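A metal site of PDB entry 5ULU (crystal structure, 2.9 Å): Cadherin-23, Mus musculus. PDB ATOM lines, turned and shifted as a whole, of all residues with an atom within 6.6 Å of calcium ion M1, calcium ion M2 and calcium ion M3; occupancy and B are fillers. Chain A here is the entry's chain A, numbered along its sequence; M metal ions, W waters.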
ATOM      1  N   GLU A 127      11.676 -29.986  24.504  1.00  0.00           N
ATOM      2  CA  GLU A 127      11.616 -28.516  24.527  1.00  0.00           C
ATOM      3  C   GLU A 127      10.895 -27.958  25.766  1.00  0.00           C
ATOM      4  O   GLU A 127      10.334 -28.710  26.589  1.00  0.00           O
ATOM      5  CB  GLU A 127      10.999 -27.952  23.225  1.00  0.00           C
ATOM      6  CG  GLU A 127       9.540 -28.314  22.960  1.00  0.00           C
ATOM      7  CD  GLU A 127       8.913 -27.500  21.823  1.00  0.00           C
ATOM      8  OE1 GLU A 127       8.193 -28.080  20.997  1.00  0.00           O
ATOM      9  OE2 GLU A 127       9.133 -26.274  21.729  1.00  0.00           O
ATOM     10  N   ASN A 128      10.978 -26.633  25.914  1.00  0.00           N
ATOM     11  CA  ASN A 128      10.351 -25.899  27.038  1.00  0.00           C
ATOM     12  C   ASN A 128      10.830 -26.331  28.403  1.00  0.00           C
ATOM     13  O   ASN A 128      10.140 -26.118  29.410  1.00  0.00           O
ATOM     14  CB  ASN A 128       8.830 -26.032  26.996  1.00  0.00           C
ATOM     15  CG  ASN A 128       8.250 -25.711  25.650  1.00  0.00           C
ATOM     16  OD1 ASN A 128       8.829 -24.969  24.836  1.00  0.00           O
ATOM     17  ND2 ASN A 128       7.072 -26.268  25.412  1.00  0.00           N
ATOM     18  N   ILE A 179      14.254 -22.811  25.449  1.00  0.00           N
ATOM     19  CA  ILE A 179      14.691 -23.591  24.319  1.00  0.00           C
ATOM     20  C   ILE A 179      13.424 -24.124  23.625  1.00  0.00           C
ATOM     21  O   ILE A 179      12.753 -25.062  24.071  1.00  0.00           O
ATOM     22  CB  ILE A 179      15.791 -24.625  24.700  1.00  0.00           C
ATOM     23  CG1 ILE A 179      15.264 -25.741  25.588  1.00  0.00           C
ATOM     24  CG2 ILE A 179      16.976 -23.934  25.378  1.00  0.00           C
ATOM     25  CD1 ILE A 179      15.025 -27.034  24.816  1.00  0.00           C
ATOM     26  N   ASP A 180      13.063 -23.407  22.574  1.00  0.00           N
ATOM     27  CA  ASP A 180      11.875 -23.685  21.769  1.00  0.00           C
ATOM     28  C   ASP A 180      12.313 -24.450  20.531  1.00  0.00           C
ATOM     29  O   ASP A 180      13.214 -23.994  19.804  1.00  0.00           O
ATOM     30  CB  ASP A 180      11.257 -22.349  21.365  1.00  0.00           C
ATOM     31  CG  ASP A 180       9.960 -22.490  20.618  1.00  0.00           C
ATOM     32  OD1 ASP A 180       9.337 -23.570  20.686  1.00  0.00           O
ATOM     33  OD2 ASP A 180       9.538 -21.487  19.986  1.00  0.00           O
ATOM     34  N   ARG A 181      11.708 -25.614  20.268  1.00  0.00           N
ATOM     35  CA  ARG A 181      12.040 -26.345  19.044  1.00  0.00           C
ATOM     36  C   ARG A 181      11.723 -25.518  17.771  1.00  0.00           C
ATOM     37  O   ARG A 181      12.492 -25.514  16.815  1.00  0.00           O
ATOM     38  CB  ARG A 181      11.337 -27.698  18.991  1.00  0.00           C
ATOM     39  CG  ARG A 181      12.055 -28.705  18.064  1.00  0.00           C
ATOM     40  CD  ARG A 181      11.163 -29.866  17.707  1.00  0.00           C
ATOM     41  NE  ARG A 181      10.043 -29.380  16.914  1.00  0.00           N
ATOM     42  CZ  ARG A 181      10.105 -29.095  15.618  1.00  0.00           C
ATOM     43  NH1 ARG A 181      11.219 -29.293  14.932  1.00  0.00           N
ATOM     44  NH2 ARG A 181       9.024 -28.607  15.016  1.00  0.00           N
ATOM     45  N   GLU A 182      10.617 -24.779  17.802  1.00  0.00           N
ATOM     46  CA  GLU A 182      10.178 -24.008  16.653  1.00  0.00           C
ATOM     47  C   GLU A 182      11.039 -22.751  16.417  1.00  0.00           C
ATOM     48  O   GLU A 182      10.902 -22.097  15.373  1.00  0.00           O
ATOM     49  CB  GLU A 182       8.702 -23.617  16.791  1.00  0.00           C
ATOM     50  CG  GLU A 182       7.698 -24.754  16.654  1.00  0.00           C
ATOM     51  CD  GLU A 182       7.689 -25.736  17.816  1.00  0.00           C
ATOM     52  OE1 GLU A 182       7.401 -26.919  17.600  1.00  0.00           O
ATOM     53  OE2 GLU A 182       7.964 -25.360  18.972  1.00  0.00           O
ATOM     54  N   GLU A 183      11.892 -22.412  17.379  1.00  0.00           N
ATOM     55  CA  GLU A 183      12.929 -21.360  17.234  1.00  0.00           C
ATOM     56  C   GLU A 183      14.177 -21.933  16.589  1.00  0.00           C
ATOM     57  O   GLU A 183      14.746 -21.339  15.694  1.00  0.00           O
ATOM     58  CB  GLU A 183      13.269 -20.769  18.619  1.00  0.00           C
ATOM     59  CG  GLU A 183      14.462 -19.824  18.759  1.00  0.00           C
ATOM     60  CD  GLU A 183      14.805 -19.597  20.238  1.00  0.00           C
ATOM     61  OE1 GLU A 183      14.617 -18.449  20.707  1.00  0.00           O
ATOM     62  OE2 GLU A 183      15.212 -20.585  20.928  1.00  0.00           O
ATOM     63  N   ASP A 212      13.727 -32.462  20.819  1.00  0.00           N
ATOM     64  CA  ASP A 212      12.483 -33.199  20.601  1.00  0.00           C
ATOM     65  C   ASP A 212      11.291 -32.273  20.711  1.00  0.00           C
ATOM     66  O   ASP A 212      11.381 -31.208  21.304  1.00  0.00           O
ATOM     67  CB  ASP A 212      12.374 -34.377  21.566  1.00  0.00           C
ATOM     68  CG  ASP A 212      13.364 -35.484  21.269  1.00  0.00           C
ATOM     69  OD1 ASP A 212      14.219 -35.321  20.351  1.00  0.00           O
ATOM     70  OD2 ASP A 212      13.290 -36.535  21.936  1.00  0.00           O
ATOM     71  N   ASP A 213      10.170 -32.691  20.143  1.00  0.00           N
ATOM     72  CA  ASP A 213       9.023 -31.821  19.988  1.00  0.00           C
ATOM     73  C   ASP A 213       7.969 -32.037  21.055  1.00  0.00           C
ATOM     74  O   ASP A 213       7.682 -33.160  21.464  1.00  0.00           O
ATOM     75  CB  ASP A 213       8.363 -32.046  18.619  1.00  0.00           C
ATOM     76  CG  ASP A 213       7.277 -31.016  18.308  1.00  0.00           C
ATOM     77  OD1 ASP A 213       7.587 -29.807  18.384  1.00  0.00           O
ATOM     78  OD2 ASP A 213       6.118 -31.427  17.993  1.00  0.00           O
ATOM     79  N   ILE A 214       7.416 -30.912  21.493  1.00  0.00           N
ATOM     80  CA  ILE A 214       6.136 -30.866  22.153  1.00  0.00           C
ATOM     81  C   ILE A 214       5.228 -30.120  21.178  1.00  0.00           C
ATOM     82  O   ILE A 214       5.651 -29.103  20.600  1.00  0.00           O
ATOM     83  CB  ILE A 214       6.233 -30.102  23.493  1.00  0.00           C
ATOM     84  CG1 ILE A 214       7.166 -30.833  24.465  1.00  0.00           C
ATOM     85  CG2 ILE A 214       4.855 -29.973  24.139  1.00  0.00           C
ATOM     86  CD1 ILE A 214       7.340 -30.139  25.797  1.00  0.00           C
ATOM     87  N   ASN A 215       4.005 -30.622  20.989  1.00  0.00           N
ATOM     88  CA  ASN A 215       3.002 -29.894  20.207  1.00  0.00           C
ATOM     89  C   ASN A 215       2.484 -28.727  21.059  1.00  0.00           C
ATOM     90  O   ASN A 215       1.458 -28.817  21.786  1.00  0.00           O
ATOM     91  CB  ASN A 215       1.894 -30.819  19.730  1.00  0.00           C
ATOM     92  CG  ASN A 215       0.950 -30.134  18.772  1.00  0.00           C
ATOM     93  OD1 ASN A 215       1.006 -28.923  18.600  1.00  0.00           O
ATOM     94  ND2 ASN A 215       0.067 -30.903  18.163  1.00  0.00           N
ATOM     95  N   ASP A 216       3.234 -27.638  20.982  1.00  0.00           N
ATOM     96  CA  ASP A 216       3.078 -26.519  21.903  1.00  0.00           C
ATOM     97  C   ASP A 216       2.798 -25.208  21.194  1.00  0.00           C
ATOM     98  O   ASP A 216       2.741 -24.166  21.843  1.00  0.00           O
ATOM     99  CB  ASP A 216       4.328 -26.411  22.807  1.00  0.00           C
ATOM    100  CG  ASP A 216       5.580 -25.943  22.061  1.00  0.00           C
ATOM    101  OD1 ASP A 216       5.623 -25.943  20.820  1.00  0.00           O
ATOM    102  OD2 ASP A 216       6.561 -25.537  22.729  1.00  0.00           O
ATOM    103  N   SER A 217       2.583 -25.267  19.871  1.00  0.00           N
ATOM    104  CA  SER A 217       2.279 -24.071  19.069  1.00  0.00           C
ATOM    105  C   SER A 217       0.813 -23.956  18.670  1.00  0.00           C
ATOM    106  O   SER A 217       0.056 -24.949  18.599  1.00  0.00           O
ATOM    107  CB  SER A 217       3.134 -23.984  17.811  1.00  0.00           C
ATOM    108  OG  SER A 217       4.447 -23.703  18.200  1.00  0.00           O
ATOM    109  N   ARG A 218       0.453 -22.718  18.397  1.00  0.00           N
ATOM    110  CA  ARG A 218      -0.886 -22.337  18.048  1.00  0.00           C
ATOM    111  C   ARG A 218      -0.987 -22.439  16.537  1.00  0.00           C
ATOM    112  O   ARG A 218      -0.131 -21.904  15.843  1.00  0.00           O
ATOM    113  CB  ARG A 218      -1.113 -20.893  18.514  1.00  0.00           C
ATOM    114  CG  ARG A 218      -2.549 -20.468  18.666  1.00  0.00           C
ATOM    115  CD  ARG A 218      -2.638 -19.081  19.282  1.00  0.00           C
ATOM    116  NE  ARG A 218      -2.229 -19.047  20.693  1.00  0.00           N
ATOM    117  CZ  ARG A 218      -2.905 -19.581  21.711  1.00  0.00           C
ATOM    118  NH1 ARG A 218      -2.397 -19.491  22.943  1.00  0.00           N
ATOM    119  NH2 ARG A 218      -4.073 -20.205  21.545  1.00  0.00           N
ATOM    120  N   PRO A 219      -2.028 -23.128  16.022  1.00  0.00           N
ATOM    121  CA  PRO A 219      -2.281 -22.951  14.600  1.00  0.00           C
ATOM    122  C   PRO A 219      -2.591 -21.508  14.368  1.00  0.00           C
ATOM    123  O   PRO A 219      -3.294 -20.937  15.171  1.00  0.00           O
ATOM    124  CB  PRO A 219      -3.541 -23.779  14.366  1.00  0.00           C
ATOM    125  CG  PRO A 219      -4.203 -23.857  15.697  1.00  0.00           C
ATOM    126  CD  PRO A 219      -3.083 -23.922  16.681  1.00  0.00           C
ATOM    127  N   ASP A 247       0.539 -24.740  11.495  1.00  0.00           N
ATOM    128  CA  ASP A 247       0.957 -25.027  12.866  1.00  0.00           C
ATOM    129  C   ASP A 247       2.353 -25.593  12.804  1.00  0.00           C
ATOM    130  O   ASP A 247       2.560 -26.695  12.325  1.00  0.00           O
ATOM    131  CB  ASP A 247       0.002 -26.030  13.550  1.00  0.00           C
ATOM    132  CG  ASP A 247       0.303 -26.197  15.045  1.00  0.00           C
ATOM    133  OD1 ASP A 247       0.429 -25.194  15.743  1.00  0.00           O
ATOM    134  OD2 ASP A 247       0.430 -27.330  15.520  1.00  0.00           O
ATOM    135  N   LEU A 248       3.311 -24.851  13.355  1.00  0.00           N
ATOM    136  CA  LEU A 248       4.729 -25.126  13.216  1.00  0.00           C
ATOM    137  C   LEU A 248       5.291 -26.320  13.993  1.00  0.00           C
ATOM    138  O   LEU A 248       6.489 -26.576  13.948  1.00  0.00           O
ATOM    139  CB  LEU A 248       5.555 -23.864  13.549  1.00  0.00           C
ATOM    140  CG  LEU A 248       5.526 -22.661  12.574  1.00  0.00           C
ATOM    141  CD1 LEU A 248       6.899 -21.999  12.528  1.00  0.00           C
ATOM    142  CD2 LEU A 248       5.124 -23.032  11.143  1.00  0.00           C
ATOM    143  N   ASP A 249       4.452 -27.078  14.674  1.00  0.00           N
ATOM    144  CA  ASP A 249       4.914 -28.311  15.294  1.00  0.00           C
ATOM    145  C   ASP A 249       5.005 -29.422  14.256  1.00  0.00           C
ATOM    146  O   ASP A 249       4.447 -29.312  13.157  1.00  0.00           O
ATOM    147  CB  ASP A 249       3.940 -28.732  16.398  1.00  0.00           C
ATOM    148  CG  ASP A 249       3.770 -27.664  17.481  1.00  0.00           C
ATOM    149  OD1 ASP A 249       4.785 -27.351  18.167  1.00  0.00           O
ATOM    150  OD2 ASP A 249       2.627 -27.150  17.649  1.00  0.00           O
ATOM    151  N   LEU A 250       5.707 -30.480  14.634  1.00  0.00           N
ATOM    152  CA  LEU A 250       5.614 -31.798  13.967  1.00  0.00           C
ATOM    153  C   LEU A 250       4.189 -32.382  14.091  1.00  0.00           C
ATOM    154  O   LEU A 250       3.549 -32.277  15.146  1.00  0.00           O
ATOM    155  CB  LEU A 250       6.588 -32.787  14.605  1.00  0.00           C
ATOM    156  CG  LEU A 250       8.047 -32.865  14.144  1.00  0.00           C
ATOM    157  CD1 LEU A 250       8.645 -31.498  13.854  1.00  0.00           C
ATOM    158  CD2 LEU A 250       8.887 -33.642  15.163  1.00  0.00           C
ATOM    159  N   PRO A 252       0.952 -31.817  13.233  1.00  0.00           N
ATOM    160  CA  PRO A 252      -0.302 -31.174  13.621  1.00  0.00           C
ATOM    161  C   PRO A 252      -1.427 -31.787  12.822  1.00  0.00           C
ATOM    162  O   PRO A 252      -1.177 -32.269  11.725  1.00  0.00           O
ATOM    163  CB  PRO A 252      -0.099 -29.734  13.185  1.00  0.00           C
ATOM    164  CG  PRO A 252       0.800 -29.823  11.998  1.00  0.00           C
ATOM    165  CD  PRO A 252       1.640 -31.056  12.186  1.00  0.00           C
ATOM    166  N   LEU A 254      -5.027 -30.129  11.905  1.00  0.00           N
ATOM    167  CA  LEU A 254      -5.921 -29.004  12.008  1.00  0.00           C
ATOM    168  C   LEU A 254      -7.313 -29.369  11.537  1.00  0.00           C
ATOM    169  O   LEU A 254      -7.474 -30.247  10.681  1.00  0.00           O
ATOM    170  CB  LEU A 254      -5.420 -27.845  11.142  1.00  0.00           C
ATOM    171  CG  LEU A 254      -3.942 -27.422  11.202  1.00  0.00           C
ATOM    172  CD1 LEU A 254      -3.713 -26.118  10.437  1.00  0.00           C
ATOM    173  CD2 LEU A 254      -3.469 -27.279  12.629  1.00  0.00           C
ATOM    174  N   ASP A 309      -5.645 -27.273  16.158  1.00  0.00           N
ATOM    175  CA  ASP A 309      -4.722 -28.378  16.031  1.00  0.00           C
ATOM    176  C   ASP A 309      -5.153 -29.417  17.048  1.00  0.00           C
ATOM    177  O   ASP A 309      -5.042 -29.187  18.244  1.00  0.00           O
ATOM    178  CB  ASP A 309      -3.290 -27.914  16.286  1.00  0.00           C
ATOM    179  CG  ASP A 309      -2.320 -29.073  16.461  1.00  0.00           C
ATOM    180  OD1 ASP A 309      -2.669 -30.236  16.123  1.00  0.00           O
ATOM    181  OD2 ASP A 309      -1.216 -28.811  16.978  1.00  0.00           O
ATOM    182  N   ALA A 311      -3.938 -32.314  17.828  1.00  0.00           N
ATOM    183  CA  ALA A 311      -2.904 -33.142  18.436  1.00  0.00           C
ATOM    184  C   ALA A 311      -2.149 -32.398  19.553  1.00  0.00           C
ATOM    185  O   ALA A 311      -1.096 -32.857  20.019  1.00  0.00           O
ATOM    186  CB  ALA A 311      -1.952 -33.612  17.358  1.00  0.00           C
ATOM    187  N   SER A 312      -2.690 -31.251  19.993  1.00  0.00           N
ATOM    188  CA  SER A 312      -1.918 -30.303  20.788  1.00  0.00           C
ATOM    189  C   SER A 312      -1.816 -30.812  22.209  1.00  0.00           C
ATOM    190  O   SER A 312      -2.807 -31.276  22.784  1.00  0.00           O
ATOM    191  CB  SER A 312      -2.509 -28.887  20.719  1.00  0.00           C
ATOM    192  OG  SER A 312      -1.519 -27.891  20.963  1.00  0.00           O
ATOM    193  N   ASP A 313      -0.611 -30.760  22.750  1.00  0.00           N
ATOM    194  CA  ASP A 313      -0.310 -31.258  24.109  1.00  0.00           C
ATOM    195  C   ASP A 313      -0.690 -30.248  25.180  1.00  0.00           C
ATOM    196  O   ASP A 313      -0.713 -30.590  26.344  1.00  0.00           O
ATOM    197  CB  ASP A 313       1.187 -31.561  24.228  1.00  0.00           C
ATOM    198  CG  ASP A 313       1.642 -32.647  23.258  1.00  0.00           C
ATOM    199  OD1 ASP A 313       0.990 -33.722  23.245  1.00  0.00           O
ATOM    200  OD2 ASP A 313       2.646 -32.436  22.532  1.00  0.00           O
ATOM    201  N   HIS A 317      -2.582 -23.713  24.058  1.00  0.00           N
ATOM    202  CA  HIS A 317      -2.002 -23.362  22.749  1.00  0.00           C
ATOM    203  C   HIS A 317      -2.654 -24.048  21.534  1.00  0.00           C
ATOM    204  O   HIS A 317      -2.080 -24.043  20.457  1.00  0.00           O
ATOM    205  CB  HIS A 317      -0.487 -23.661  22.769  1.00  0.00           C
ATOM    206  CG  HIS A 317       0.296 -22.699  23.601  1.00  0.00           C
ATOM    207  ND1 HIS A 317       0.038 -21.348  23.612  1.00  0.00           N
ATOM    208  CD2 HIS A 317       1.345 -22.890  24.419  1.00  0.00           C
ATOM    209  CE1 HIS A 317       0.890 -20.746  24.422  1.00  0.00           C
ATOM    210  NE2 HIS A 317       1.695 -21.662  24.918  1.00  0.00           N
ATOM    211  N   SER A 318      -3.847 -24.587  21.693  1.00  0.00           N
ATOM    212  CA  SER A 318      -4.379 -25.492  20.687  1.00  0.00           C
ATOM    213  C   SER A 318      -5.376 -24.853  19.716  1.00  0.00           C
ATOM    214  O   SER A 318      -5.986 -25.578  18.955  1.00  0.00           O
ATOM    215  CB  SER A 318      -5.013 -26.705  21.356  1.00  0.00           C
ATOM    216  OG  SER A 318      -6.346 -26.442  21.726  1.00  0.00           O
HETATM  217 CA    CA M   1       0.061 -27.191  17.690  1.00  0.00          CA
HETATM  218 CA    CA M   2       6.723 -27.777  19.325  1.00  0.00          CA
HETATM  219 CA    CA M   3       7.589 -24.383  21.103  1.00  0.00          CA
HETATM  220  O   HOH W   1       8.329 -22.062  23.303  1.00  0.00           O
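Calcium ion M2 is bound by OE1 of Glu 182 (2.0 Å), O of Ile 214 (2.1 Å), OE1 of Glu 127 (2.2 Å), OD1 of Asp 249 (2.3 Å), OD1 of Asp 213 (2.4 Å), OD1 of Asp 216 (2.6 Å) and OE2 of Glu 182 (2.7 Å).
Six residues have an atom within 4 Å of calcium ion M2: Glu 127, Glu 182, Asp 213, Ile 214, Asp 216 and Asp 249.
Calcium ion M1 is bound by the side-chain amide oxygen (OD1) of Asn 215, the side-chain carboxylate (OD2) of Asp 309, the side-chain carboxylate (OD2) of Asp 247, the backbone carbonyl oxygen (O) of Ser 217, the side-chain carboxylate (OD2) of Asp 249 and the side-chain carboxylate (OD1) of Asp 247. Calcium ion M1 has six donor atoms within binding distance.
Merely in contact with calcium ion M1: Ser 312 (3.7 Å). Six residues have an atom within 4 Å of calcium ion M1: Asn 215, Ser 217, Asp 247, Asp 249, Asp 309 and Ser 312. Along chain A the residues within 4 Å of calcium ion M1 span positions 215 to 312. The nearest printed residue that does not touch calcium ion M1 is Arg 218 (4.5 Å).
Calcium ion M3 is bound by OD1 of Asp 180 (2.0 Å), OD2 of Asp 216 (2.2 Å), OE2 of Glu 182 (2.4 Å), OE2 of Glu 127 (2.5 Å) and OD1 of Asp 216 (2.5 Å). Calcium ion M3 has five donor atoms within binding distance.
Merely in contact with calcium ion M3: Asn 128. The nearest printed residue that does not touch calcium ion M3 is Ser 217 (4.3 Å).
The side-chain carboxylate of Asp 213 sits close to the guanidinium group of Arg 181 (2.9 Å). N of Asp 309 lies within hydrogen-bond range of O of Ser 318, at 3.3 Å. The side-chain carboxylate of Asp 309 lies within hydrogen-bond range of the backbone NH of Ala 311 (3.0 Å). The side-chain amide nitrogen (ND2) of Asn 128 sits close to the side-chain carboxylate (OD2) of Asp 216. The side-chain hydroxyl (OG) of Ser 312 is in hydrogen-bond range of the backbone carbonyl oxygen (O) of Asn 215 (3.2 Å). OE1 of Glu 182 sits close to NH2 of Arg 181 (3.5 Å). The backbone NH (N) of Glu 127 lies within hydrogen-bond range of the backbone carbonyl oxygen (O) of Asp 212, at 3.4 Å. N of Asn 128 lies within hydrogen-bond range of O of Ile 179 (3.0 Å).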
